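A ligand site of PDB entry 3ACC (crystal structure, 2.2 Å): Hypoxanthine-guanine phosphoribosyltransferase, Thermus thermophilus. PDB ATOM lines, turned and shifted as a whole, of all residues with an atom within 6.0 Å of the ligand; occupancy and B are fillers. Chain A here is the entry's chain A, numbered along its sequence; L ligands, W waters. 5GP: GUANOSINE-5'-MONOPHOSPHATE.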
ATOM      1  N   VAL A  44       6.599 -34.738  17.402  1.00  0.00           N
ATOM      2  CA  VAL A  44       5.161 -34.618  17.175  1.00  0.00           C
ATOM      3  C   VAL A  44       4.954 -34.278  15.709  1.00  0.00           C
ATOM      4  O   VAL A  44       5.211 -33.151  15.280  1.00  0.00           O
ATOM      5  CB  VAL A  44       4.530 -33.515  18.067  1.00  0.00           C
ATOM      6  CG1 VAL A  44       3.031 -33.423  17.819  1.00  0.00           C
ATOM      7  CG2 VAL A  44       4.779 -33.826  19.538  1.00  0.00           C
ATOM      8  N   GLY A  47       4.259 -31.290  11.732  1.00  0.00           N
ATOM      9  CA  GLY A  47       4.988 -30.040  11.791  1.00  0.00           C
ATOM     10  C   GLY A  47       6.393 -29.956  12.371  1.00  0.00           C
ATOM     11  O   GLY A  47       7.168 -29.083  11.975  1.00  0.00           O
ATOM     12  N   SER A  72      -6.006 -31.705  18.421  1.00  0.00           N
ATOM     13  CA  SER A  72      -6.691 -31.023  19.515  1.00  0.00           C
ATOM     14  C   SER A  72      -8.023 -31.693  19.867  1.00  0.00           C
ATOM     15  O   SER A  72      -8.807 -32.052  18.993  1.00  0.00           O
ATOM     16  CB  SER A  72      -6.941 -29.563  19.144  1.00  0.00           C
ATOM     17  OG  SER A  72      -7.478 -28.836  20.238  1.00  0.00           O
ATOM     18  N   GLU A 102       8.254 -30.486  19.679  1.00  0.00           N
ATOM     19  CA  GLU A 102       7.079 -29.880  19.086  1.00  0.00           C
ATOM     20  C   GLU A 102       7.415 -28.754  18.099  1.00  0.00           C
ATOM     21  O   GLU A 102       8.527 -28.207  18.135  1.00  0.00           O
ATOM     22  CB  GLU A 102       6.218 -29.320  20.227  1.00  0.00           C
ATOM     23  CG  GLU A 102       4.879 -28.819  19.783  1.00  0.00           C
ATOM     24  CD  GLU A 102       3.998 -29.937  19.310  1.00  0.00           C
ATOM     25  OE1 GLU A 102       3.454 -30.668  20.164  1.00  0.00           O
ATOM     26  OE2 GLU A 102       3.848 -30.091  18.078  1.00  0.00           O
ATOM     27  N   ASP A 103       6.471 -28.409  17.226  1.00  0.00           N
ATOM     28  CA  ASP A 103       6.713 -27.331  16.270  1.00  0.00           C
ATOM     29  C   ASP A 103       6.410 -25.972  16.888  1.00  0.00           C
ATOM     30  O   ASP A 103       7.287 -25.106  16.987  1.00  0.00           O
ATOM     31  CB  ASP A 103       5.883 -27.532  14.990  1.00  0.00           C
ATOM     32  CG  ASP A 103       4.408 -27.755  15.247  1.00  0.00           C
ATOM     33  OD1 ASP A 103       3.983 -27.844  16.424  1.00  0.00           O
ATOM     34  OD2 ASP A 103       3.641 -27.858  14.252  1.00  0.00           O
ATOM     35  N   ILE A 104       5.173 -25.767  17.330  1.00  0.00           N
ATOM     36  CA  ILE A 104       4.808 -24.501  17.940  1.00  0.00           C
ATOM     37  C   ILE A 104       3.701 -24.683  18.959  1.00  0.00           C
ATOM     38  O   ILE A 104       2.789 -25.485  18.777  1.00  0.00           O
ATOM     39  CB  ILE A 104       4.355 -23.493  16.851  1.00  0.00           C
ATOM     40  CG1 ILE A 104       3.891 -22.191  17.495  1.00  0.00           C
ATOM     41  CG2 ILE A 104       3.248 -24.111  15.987  1.00  0.00           C
ATOM     42  CD1 ILE A 104       3.668 -21.069  16.496  1.00  0.00           C
ATOM     43  N   VAL A 105       3.796 -23.951  20.068  1.00  0.00           N
ATOM     44  CA  VAL A 105       2.797 -24.012  21.123  1.00  0.00           C
ATOM     45  C   VAL A 105       1.881 -22.809  20.992  1.00  0.00           C
ATOM     46  O   VAL A 105       2.315 -21.664  21.144  1.00  0.00           O
ATOM     47  CB  VAL A 105       3.462 -24.009  22.514  1.00  0.00           C
ATOM     48  CG1 VAL A 105       2.384 -24.035  23.617  1.00  0.00           C
ATOM     49  CG2 VAL A 105       4.407 -25.214  22.638  1.00  0.00           C
ATOM     50  N   ASP A 106       0.606 -23.072  20.702  1.00  0.00           N
ATOM     51  CA  ASP A 106      -0.384 -22.015  20.524  1.00  0.00           C
ATOM     52  C   ASP A 106      -1.212 -21.878  21.809  1.00  0.00           C
ATOM     53  O   ASP A 106      -0.804 -21.178  22.746  1.00  0.00           O
ATOM     54  CB  ASP A 106      -1.266 -22.354  19.320  1.00  0.00           C
ATOM     55  CG  ASP A 106      -2.164 -21.216  18.898  1.00  0.00           C
ATOM     56  OD1 ASP A 106      -1.864 -20.045  19.223  1.00  0.00           O
ATOM     57  OD2 ASP A 106      -3.172 -21.483  18.221  1.00  0.00           O
ATOM     58  N   THR A 107      -2.370 -22.522  21.862  1.00  0.00           N
ATOM     59  CA  THR A 107      -3.198 -22.435  23.068  1.00  0.00           C
ATOM     60  C   THR A 107      -2.588 -23.319  24.160  1.00  0.00           C
ATOM     61  O   THR A 107      -2.810 -23.088  25.344  1.00  0.00           O
ATOM     62  CB  THR A 107      -4.648 -22.918  22.827  1.00  0.00           C
ATOM     63  OG1 THR A 107      -4.652 -24.310  22.502  1.00  0.00           O
ATOM     64  CG2 THR A 107      -5.293 -22.127  21.690  1.00  0.00           C
ATOM     65  N   GLY A 108      -1.814 -24.319  23.730  1.00  0.00           N
ATOM     66  CA  GLY A 108      -1.184 -25.238  24.666  1.00  0.00           C
ATOM     67  C   GLY A 108      -2.002 -26.496  24.949  1.00  0.00           C
ATOM     68  O   GLY A 108      -1.550 -27.403  25.642  1.00  0.00           O
ATOM     69  N   LEU A 109      -3.207 -26.539  24.398  1.00  0.00           N
ATOM     70  CA  LEU A 109      -4.118 -27.674  24.583  1.00  0.00           C
ATOM     71  C   LEU A 109      -3.499 -29.000  24.163  1.00  0.00           C
ATOM     72  O   LEU A 109      -3.443 -29.946  24.940  1.00  0.00           O
ATOM     73  CB  LEU A 109      -5.419 -27.451  23.797  1.00  0.00           C
ATOM     74  CG  LEU A 109      -6.752 -27.732  24.499  1.00  0.00           C
ATOM     75  CD1 LEU A 109      -7.857 -27.810  23.458  1.00  0.00           C
ATOM     76  CD2 LEU A 109      -6.682 -29.028  25.279  1.00  0.00           C
ATOM     77  N   THR A 110      -3.040 -29.073  22.912  1.00  0.00           N
ATOM     78  CA  THR A 110      -2.446 -30.300  22.390  1.00  0.00           C
ATOM     79  C   THR A 110      -1.291 -30.802  23.244  1.00  0.00           C
ATOM     80  O   THR A 110      -1.243 -31.972  23.611  1.00  0.00           O
ATOM     81  CB  THR A 110      -1.950 -30.102  20.941  1.00  0.00           C
ATOM     82  OG1 THR A 110      -3.051 -29.751  20.104  1.00  0.00           O
ATOM     83  CG2 THR A 110      -1.323 -31.380  20.420  1.00  0.00           C
ATOM     84  N   LEU A 111      -0.342 -29.920  23.553  1.00  0.00           N
ATOM     85  CA  LEU A 111       0.795 -30.316  24.372  1.00  0.00           C
ATOM     86  C   LEU A 111       0.351 -30.764  25.755  1.00  0.00           C
ATOM     87  O   LEU A 111       0.942 -31.665  26.339  1.00  0.00           O
ATOM     88  CB  LEU A 111       1.790 -29.148  24.499  1.00  0.00           C
ATOM     89  CG  LEU A 111       3.040 -29.441  25.339  1.00  0.00           C
ATOM     90  CD1 LEU A 111       3.751 -30.679  24.793  1.00  0.00           C
ATOM     91  CD2 LEU A 111       3.955 -28.229  25.306  1.00  0.00           C
ATOM     92  N   LYS A 134       3.524 -18.958  21.033  1.00  0.00           N
ATOM     93  CA  LYS A 134       2.720 -17.737  20.973  1.00  0.00           C
ATOM     94  C   LYS A 134       1.987 -17.629  22.320  1.00  0.00           C
ATOM     95  O   LYS A 134       0.782 -17.850  22.395  1.00  0.00           O
ATOM     96  CB  LYS A 134       1.727 -17.813  19.805  1.00  0.00           C
ATOM     97  CG  LYS A 134       2.397 -17.926  18.433  1.00  0.00           C
ATOM     98  CD  LYS A 134       1.392 -18.050  17.281  1.00  0.00           C
ATOM     99  CE  LYS A 134       0.612 -19.369  17.340  1.00  0.00           C
ATOM    100  NZ  LYS A 134      -0.280 -19.531  16.155  1.00  0.00           N
ATOM    101  N   ARG A 137      -1.571 -16.377  23.241  1.00  0.00           N
ATOM    102  CA  ARG A 137      -2.683 -17.260  22.901  1.00  0.00           C
ATOM    103  C   ARG A 137      -2.850 -18.404  23.904  1.00  0.00           C
ATOM    104  O   ARG A 137      -3.792 -19.180  23.820  1.00  0.00           O
ATOM    105  CB  ARG A 137      -2.430 -17.855  21.506  1.00  0.00           C
ATOM    106  CG  ARG A 137      -2.543 -16.854  20.364  1.00  0.00           C
ATOM    107  CD  ARG A 137      -3.923 -16.914  19.743  1.00  0.00           C
ATOM    108  NE  ARG A 137      -4.220 -18.268  19.268  1.00  0.00           N
ATOM    109  CZ  ARG A 137      -5.395 -18.664  18.786  1.00  0.00           C
ATOM    110  NH1 ARG A 137      -6.403 -17.810  18.703  1.00  0.00           N
ATOM    111  NH2 ARG A 137      -5.558 -19.922  18.386  1.00  0.00           N
ATOM    112  N   ARG A 138      -1.927 -18.480  24.864  1.00  0.00           N
ATOM    113  CA  ARG A 138      -1.939 -19.537  25.870  1.00  0.00           C
ATOM    114  C   ARG A 138      -3.213 -19.612  26.719  1.00  0.00           C
ATOM    115  O   ARG A 138      -3.621 -18.627  27.332  1.00  0.00           O
ATOM    116  CB  ARG A 138      -0.701 -19.390  26.776  1.00  0.00           C
ATOM    117  CG  ARG A 138      -0.263 -20.662  27.506  1.00  0.00           C
ATOM    118  CD  ARG A 138      -0.081 -21.839  26.538  1.00  0.00           C
ATOM    119  NE  ARG A 138       0.471 -21.405  25.256  1.00  0.00           N
ATOM    120  CZ  ARG A 138       1.737 -21.032  25.058  1.00  0.00           C
ATOM    121  NH1 ARG A 138       2.599 -21.060  26.063  1.00  0.00           N
ATOM    122  NH2 ARG A 138       2.122 -20.618  23.854  1.00  0.00           N
ATOM    123  N   ALA A 154       0.327 -14.878  15.401  1.00  0.00           N
ATOM    124  CA  ALA A 154       0.256 -14.863  13.938  1.00  0.00           C
ATOM    125  C   ALA A 154       0.290 -16.297  13.427  1.00  0.00           C
ATOM    126  O   ALA A 154       0.791 -17.190  14.102  1.00  0.00           O
ATOM    127  CB  ALA A 154       1.441 -14.089  13.367  1.00  0.00           C
ATOM    128  N   TYR A 155      -0.267 -16.529  12.242  1.00  0.00           N
ATOM    129  CA  TYR A 155      -0.240 -17.873  11.694  1.00  0.00           C
ATOM    130  C   TYR A 155       1.014 -18.001  10.853  1.00  0.00           C
ATOM    131  O   TYR A 155       1.112 -17.427   9.760  1.00  0.00           O
ATOM    132  CB  TYR A 155      -1.479 -18.168  10.848  1.00  0.00           C
ATOM    133  CG  TYR A 155      -1.554 -19.619  10.418  1.00  0.00           C
ATOM    134  CD1 TYR A 155      -0.852 -20.087   9.306  1.00  0.00           C
ATOM    135  CD2 TYR A 155      -2.277 -20.550  11.167  1.00  0.00           C
ATOM    136  CE1 TYR A 155      -0.883 -21.429   8.938  1.00  0.00           C
ATOM    137  CE2 TYR A 155      -2.312 -21.898  10.818  1.00  0.00           C
ATOM    138  CZ  TYR A 155      -1.608 -22.326   9.697  1.00  0.00           C
ATOM    139  OH  TYR A 155      -1.621 -23.661   9.366  1.00  0.00           O
ATOM    140  N   VAL A 156       1.972 -18.751  11.372  1.00  0.00           N
ATOM    141  CA  VAL A 156       3.243 -18.968  10.700  1.00  0.00           C
ATOM    142  C   VAL A 156       3.221 -20.256   9.893  1.00  0.00           C
ATOM    143  O   VAL A 156       2.306 -21.061  10.017  1.00  0.00           O
ATOM    144  CB  VAL A 156       4.395 -19.026  11.719  1.00  0.00           C
ATOM    145  CG1 VAL A 156       4.420 -17.740  12.557  1.00  0.00           C
ATOM    146  CG2 VAL A 156       4.218 -20.237  12.637  1.00  0.00           C
ATOM    147  N   TYR A 157       4.231 -20.435   9.054  1.00  0.00           N
ATOM    148  CA  TYR A 157       4.357 -21.642   8.247  1.00  0.00           C
ATOM    149  C   TYR A 157       5.779 -21.710   7.712  1.00  0.00           C
ATOM    150  O   TYR A 157       6.524 -20.736   7.776  1.00  0.00           O
ATOM    151  CB  TYR A 157       3.326 -21.666   7.120  1.00  0.00           C
ATOM    152  CG  TYR A 157       3.416 -20.541   6.118  1.00  0.00           C
ATOM    153  CD1 TYR A 157       4.156 -20.684   4.941  1.00  0.00           C
ATOM    154  CD2 TYR A 157       2.725 -19.344   6.326  1.00  0.00           C
ATOM    155  CE1 TYR A 157       4.204 -19.661   3.995  1.00  0.00           C
ATOM    156  CE2 TYR A 157       2.767 -18.313   5.381  1.00  0.00           C
ATOM    157  CZ  TYR A 157       3.515 -18.479   4.221  1.00  0.00           C
ATOM    158  OH  TYR A 157       3.551 -17.477   3.277  1.00  0.00           O
ATOM    159  N   LEU A 161       6.241 -26.519   9.184  1.00  0.00           N
ATOM    160  CA  LEU A 161       4.869 -26.086   9.457  1.00  0.00           C
ATOM    161  C   LEU A 161       4.149 -25.769   8.152  1.00  0.00           C
ATOM    162  O   LEU A 161       4.717 -25.170   7.231  1.00  0.00           O
ATOM    163  CB  LEU A 161       4.862 -24.864  10.387  1.00  0.00           C
ATOM    164  CG  LEU A 161       5.353 -25.117  11.816  1.00  0.00           C
ATOM    165  CD1 LEU A 161       6.850 -25.407  11.823  1.00  0.00           C
ATOM    166  CD2 LEU A 161       5.062 -23.902  12.680  1.00  0.00           C
ATOM    167  N   ASP A 162       2.891 -26.167   8.079  1.00  0.00           N
ATOM    168  CA  ASP A 162       2.110 -25.982   6.861  1.00  0.00           C
ATOM    169  C   ASP A 162       1.130 -24.829   6.820  1.00  0.00           C
ATOM    170  O   ASP A 162       0.819 -24.186   7.826  1.00  0.00           O
ATOM    171  CB  ASP A 162       1.340 -27.261   6.573  1.00  0.00           C
ATOM    172  CG  ASP A 162       0.163 -27.444   7.514  1.00  0.00           C
ATOM    173  OD1 ASP A 162       0.399 -27.475   8.739  1.00  0.00           O
ATOM    174  OD2 ASP A 162      -0.983 -27.546   7.042  1.00  0.00           O
ATOM    175  N   ARG A 163       0.622 -24.622   5.607  1.00  0.00           N
ATOM    176  CA  ARG A 163      -0.388 -23.636   5.309  1.00  0.00           C
ATOM    177  C   ARG A 163      -1.284 -24.456   4.403  1.00  0.00           C
ATOM    178  O   ARG A 163      -1.034 -24.563   3.197  1.00  0.00           O
ATOM    179  CB  ARG A 163       0.222 -22.439   4.565  1.00  0.00           C
ATOM    180  CG  ARG A 163      -0.773 -21.322   4.298  1.00  0.00           C
ATOM    181  CD  ARG A 163      -0.092 -20.061   3.779  1.00  0.00           C
ATOM    182  NE  ARG A 163       0.746 -20.323   2.617  1.00  0.00           N
ATOM    183  CZ  ARG A 163       1.172 -19.380   1.772  1.00  0.00           C
ATOM    184  NH1 ARG A 163       0.830 -18.117   1.971  1.00  0.00           N
ATOM    185  NH2 ARG A 163       1.935 -19.706   0.747  1.00  0.00           N
HETATM  186  P   5GP L   1      -2.213 -25.766  20.340  1.00  0.00           P
HETATM  187  O1P 5GP L   1      -3.291 -24.748  20.389  1.00  0.00           O
HETATM  188  O2P 5GP L   1      -2.793 -27.157  20.883  1.00  0.00           O
HETATM  189  O3P 5GP L   1      -0.988 -25.310  21.274  1.00  0.00           O
HETATM  190  O5' 5GP L   1      -1.705 -25.882  18.809  1.00  0.00           O
HETATM  191  C5' 5GP L   1      -1.206 -27.203  18.591  1.00  0.00           C
HETATM  192  C4' 5GP L   1      -0.894 -27.393  17.107  1.00  0.00           C
HETATM  193  O4' 5GP L   1      -1.589 -26.404  16.285  1.00  0.00           O
HETATM  194  C3' 5GP L   1       0.605 -27.138  16.832  1.00  0.00           C
HETATM  195  O3' 5GP L   1       1.385 -28.302  17.118  1.00  0.00           O
HETATM  196  C2' 5GP L   1       0.601 -26.820  15.335  1.00  0.00           C
HETATM  197  O2' 5GP L   1       0.599 -28.008  14.530  1.00  0.00           O
HETATM  198  C1' 5GP L   1      -0.730 -26.036  15.169  1.00  0.00           C
HETATM  199  N9  5GP L   1      -0.458 -24.593  15.072  1.00  0.00           N
HETATM  200  C8  5GP L   1      -0.646 -23.629  16.028  1.00  0.00           C
HETATM  201  N7  5GP L   1      -0.281 -22.458  15.569  1.00  0.00           N
HETATM  202  C5  5GP L   1       0.165 -22.600  14.305  1.00  0.00           C
HETATM  203  C6  5GP L   1       0.693 -21.719  13.302  1.00  0.00           C
HETATM  204  O6  5GP L   1       0.815 -20.524  13.526  1.00  0.00           O
HETATM  205  N1  5GP L   1       1.055 -22.241  12.088  1.00  0.00           N
HETATM  206  C2  5GP L   1       0.920 -23.590  11.836  1.00  0.00           C
HETATM  207  N2  5GP L   1       1.292 -24.104  10.616  1.00  0.00           N
HETATM  208  N3  5GP L   1       0.438 -24.411  12.749  1.00  0.00           N
HETATM  209  C4  5GP L   1       0.066 -23.972  13.968  1.00  0.00           C
HETATM  210  O   HOH W   1      -5.378 -27.116  20.116  1.00  0.00           O
HETATM  211  O   HOH W   2       0.342 -27.311  22.336  1.00  0.00           O
HETATM  212  O   HOH W   3       2.120 -27.673  20.378  1.00  0.00           O
HETATM  213  O   HOH W   4      -1.309 -29.059  13.159  1.00  0.00           O
HETATM  214  O   HOH W   5       2.250 -26.933  11.899  1.00  0.00           O
HETATM  215  O   HOH W   6      -4.406 -23.800  18.127  1.00  0.00           O
HETATM  216  O   HOH W   7       1.139 -30.354  19.149  1.00  0.00           O
HETATM  217  O   HOH W   8      -2.930 -20.822  15.186  1.00  0.00           O
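The backbone NH (N) of Thr 107 lies within hydrogen-bond range of an oxygen (O1P) of the ligand (2.8 Å). The side-chain hydroxyl (OG1) of Thr 107 is in hydrogen-bond range of an oxygen (O1P) of the ligand (2.6 Å). An oxygen (O6) of the ligand sits at hydrogen-bond distance from the backbone NH (N) of Val 156 (3.0 Å). The backbone carbonyl oxygen (O) of Val 156 lies within hydrogen-bond range of a nitrogen (N1) of the ligand. The backbone NH (N) of Thr 110 lies within hydrogen-bond range of an oxygen (O2P) of the ligand. An oxygen (O2P) of the ligand is in hydrogen-bond range of the side-chain hydroxyl (OG1) of Thr 110 (2.7 Å). The side-chain carboxylate (OD1) of Asp 103 lies within hydrogen-bond range of an oxygen (O3') of the ligand (2.7 Å). N of Gly 108 sits at hydrogen-bond distance from O3P of the ligand, at 2.8 Å. The backbone NH (N) of Asp 106 lies within hydrogen-bond range of an oxygen (O3P) of the ligand (2.8 Å). A nitrogen (N2) of the ligand lies within hydrogen-bond range of the backbone carbonyl oxygen (O) of Asp 162 (2.8 Å). The side-chain amino group of Lys 134 is in hydrogen-bond range of a nitrogen (N7) of the ligand (3.0 Å). O3' of the ligand lies within hydrogen-bond range of OE2 of Glu 102. OH of Tyr 155 is in hydrogen-bond range of N2 of the ligand (3.2 Å).
The side-chain hydroxyl (OG1) of Thr 107 is in hydrogen-bond range of the backbone NH (N) of Leu 109 (3.3 Å). The side-chain carboxylate of Asp 106 lies within salt-bridge range of the side-chain amino group of Lys 134 (3.5 Å). The side-chain carboxylate of Asp 106 lies within salt-bridge range of the guanidinium group of Arg 137 (2.9 Å). O of Asp 106 is in hydrogen-bond range of NE of Arg 138 (2.8 Å). O of Asp 162 sits at hydrogen-bond distance from OH of Tyr 155, at 2.9 Å. The backbone carbonyl oxygen (O) of Ala 154 sits at hydrogen-bond distance from the side-chain amino group (NZ) of Lys 134, 3.3 Å away. NH2 of Arg 138 lies close to O of Lys 134 (3.4 Å). The backbone carbonyl oxygen of Val 105 is in hydrogen-bond range of the guanidinium group of Arg 138, 2.9 Å away.
An oxygen (O6) of the ligand sits close to the backbone carbonyl oxygen (O) of Ala 154. Residues that only touch the ligand: Ile 104 (3.4 Å), Leu 109 (3.6 Å), Leu 161 (3.7 Å) and Val 105 (3.8 Å). Hydrophobic or aromatic side chains within 4 Å of the ligand: Ile 104, Leu 109, Tyr 155, Val 156 and Leu 161. Within 4 Å of the ligand: Glu 102, Asp 103, Ile 104, Val 105, Asp 106, Thr 107, Gly 108, Leu 109, Thr 110, Lys 134, Ala 154, Tyr 155, Val 156, Leu 161 and Asp 162.
Water W2 bridges an oxygen (O3P) of the ligand (2.6 Å) and the backbone NH of Leu 111 (3.0 Å). Water W6 lies within hydrogen-bond range of the side-chain carboxylate (OD2) of Asp 106 and an oxygen (O1P) of the ligand. Water W1 lies within hydrogen-bond range of O2P of the ligand (2.7 Å) and OG of Ser 72 (2.7 Å). Water W7 lies within hydrogen-bond range of OE1 of Glu 102 (2.5 Å) and O3' of the ligand (2.9 Å). Water W8 lies within hydrogen-bond range of NZ of Lys 134, OD2 of Asp 106 and N7 of the ligand. Water W5 lies within hydrogen-bond range of the side-chain carboxylate of Asp 103 (2.9 Å) and a nitrogen (N3) of the ligand (3.2 Å).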
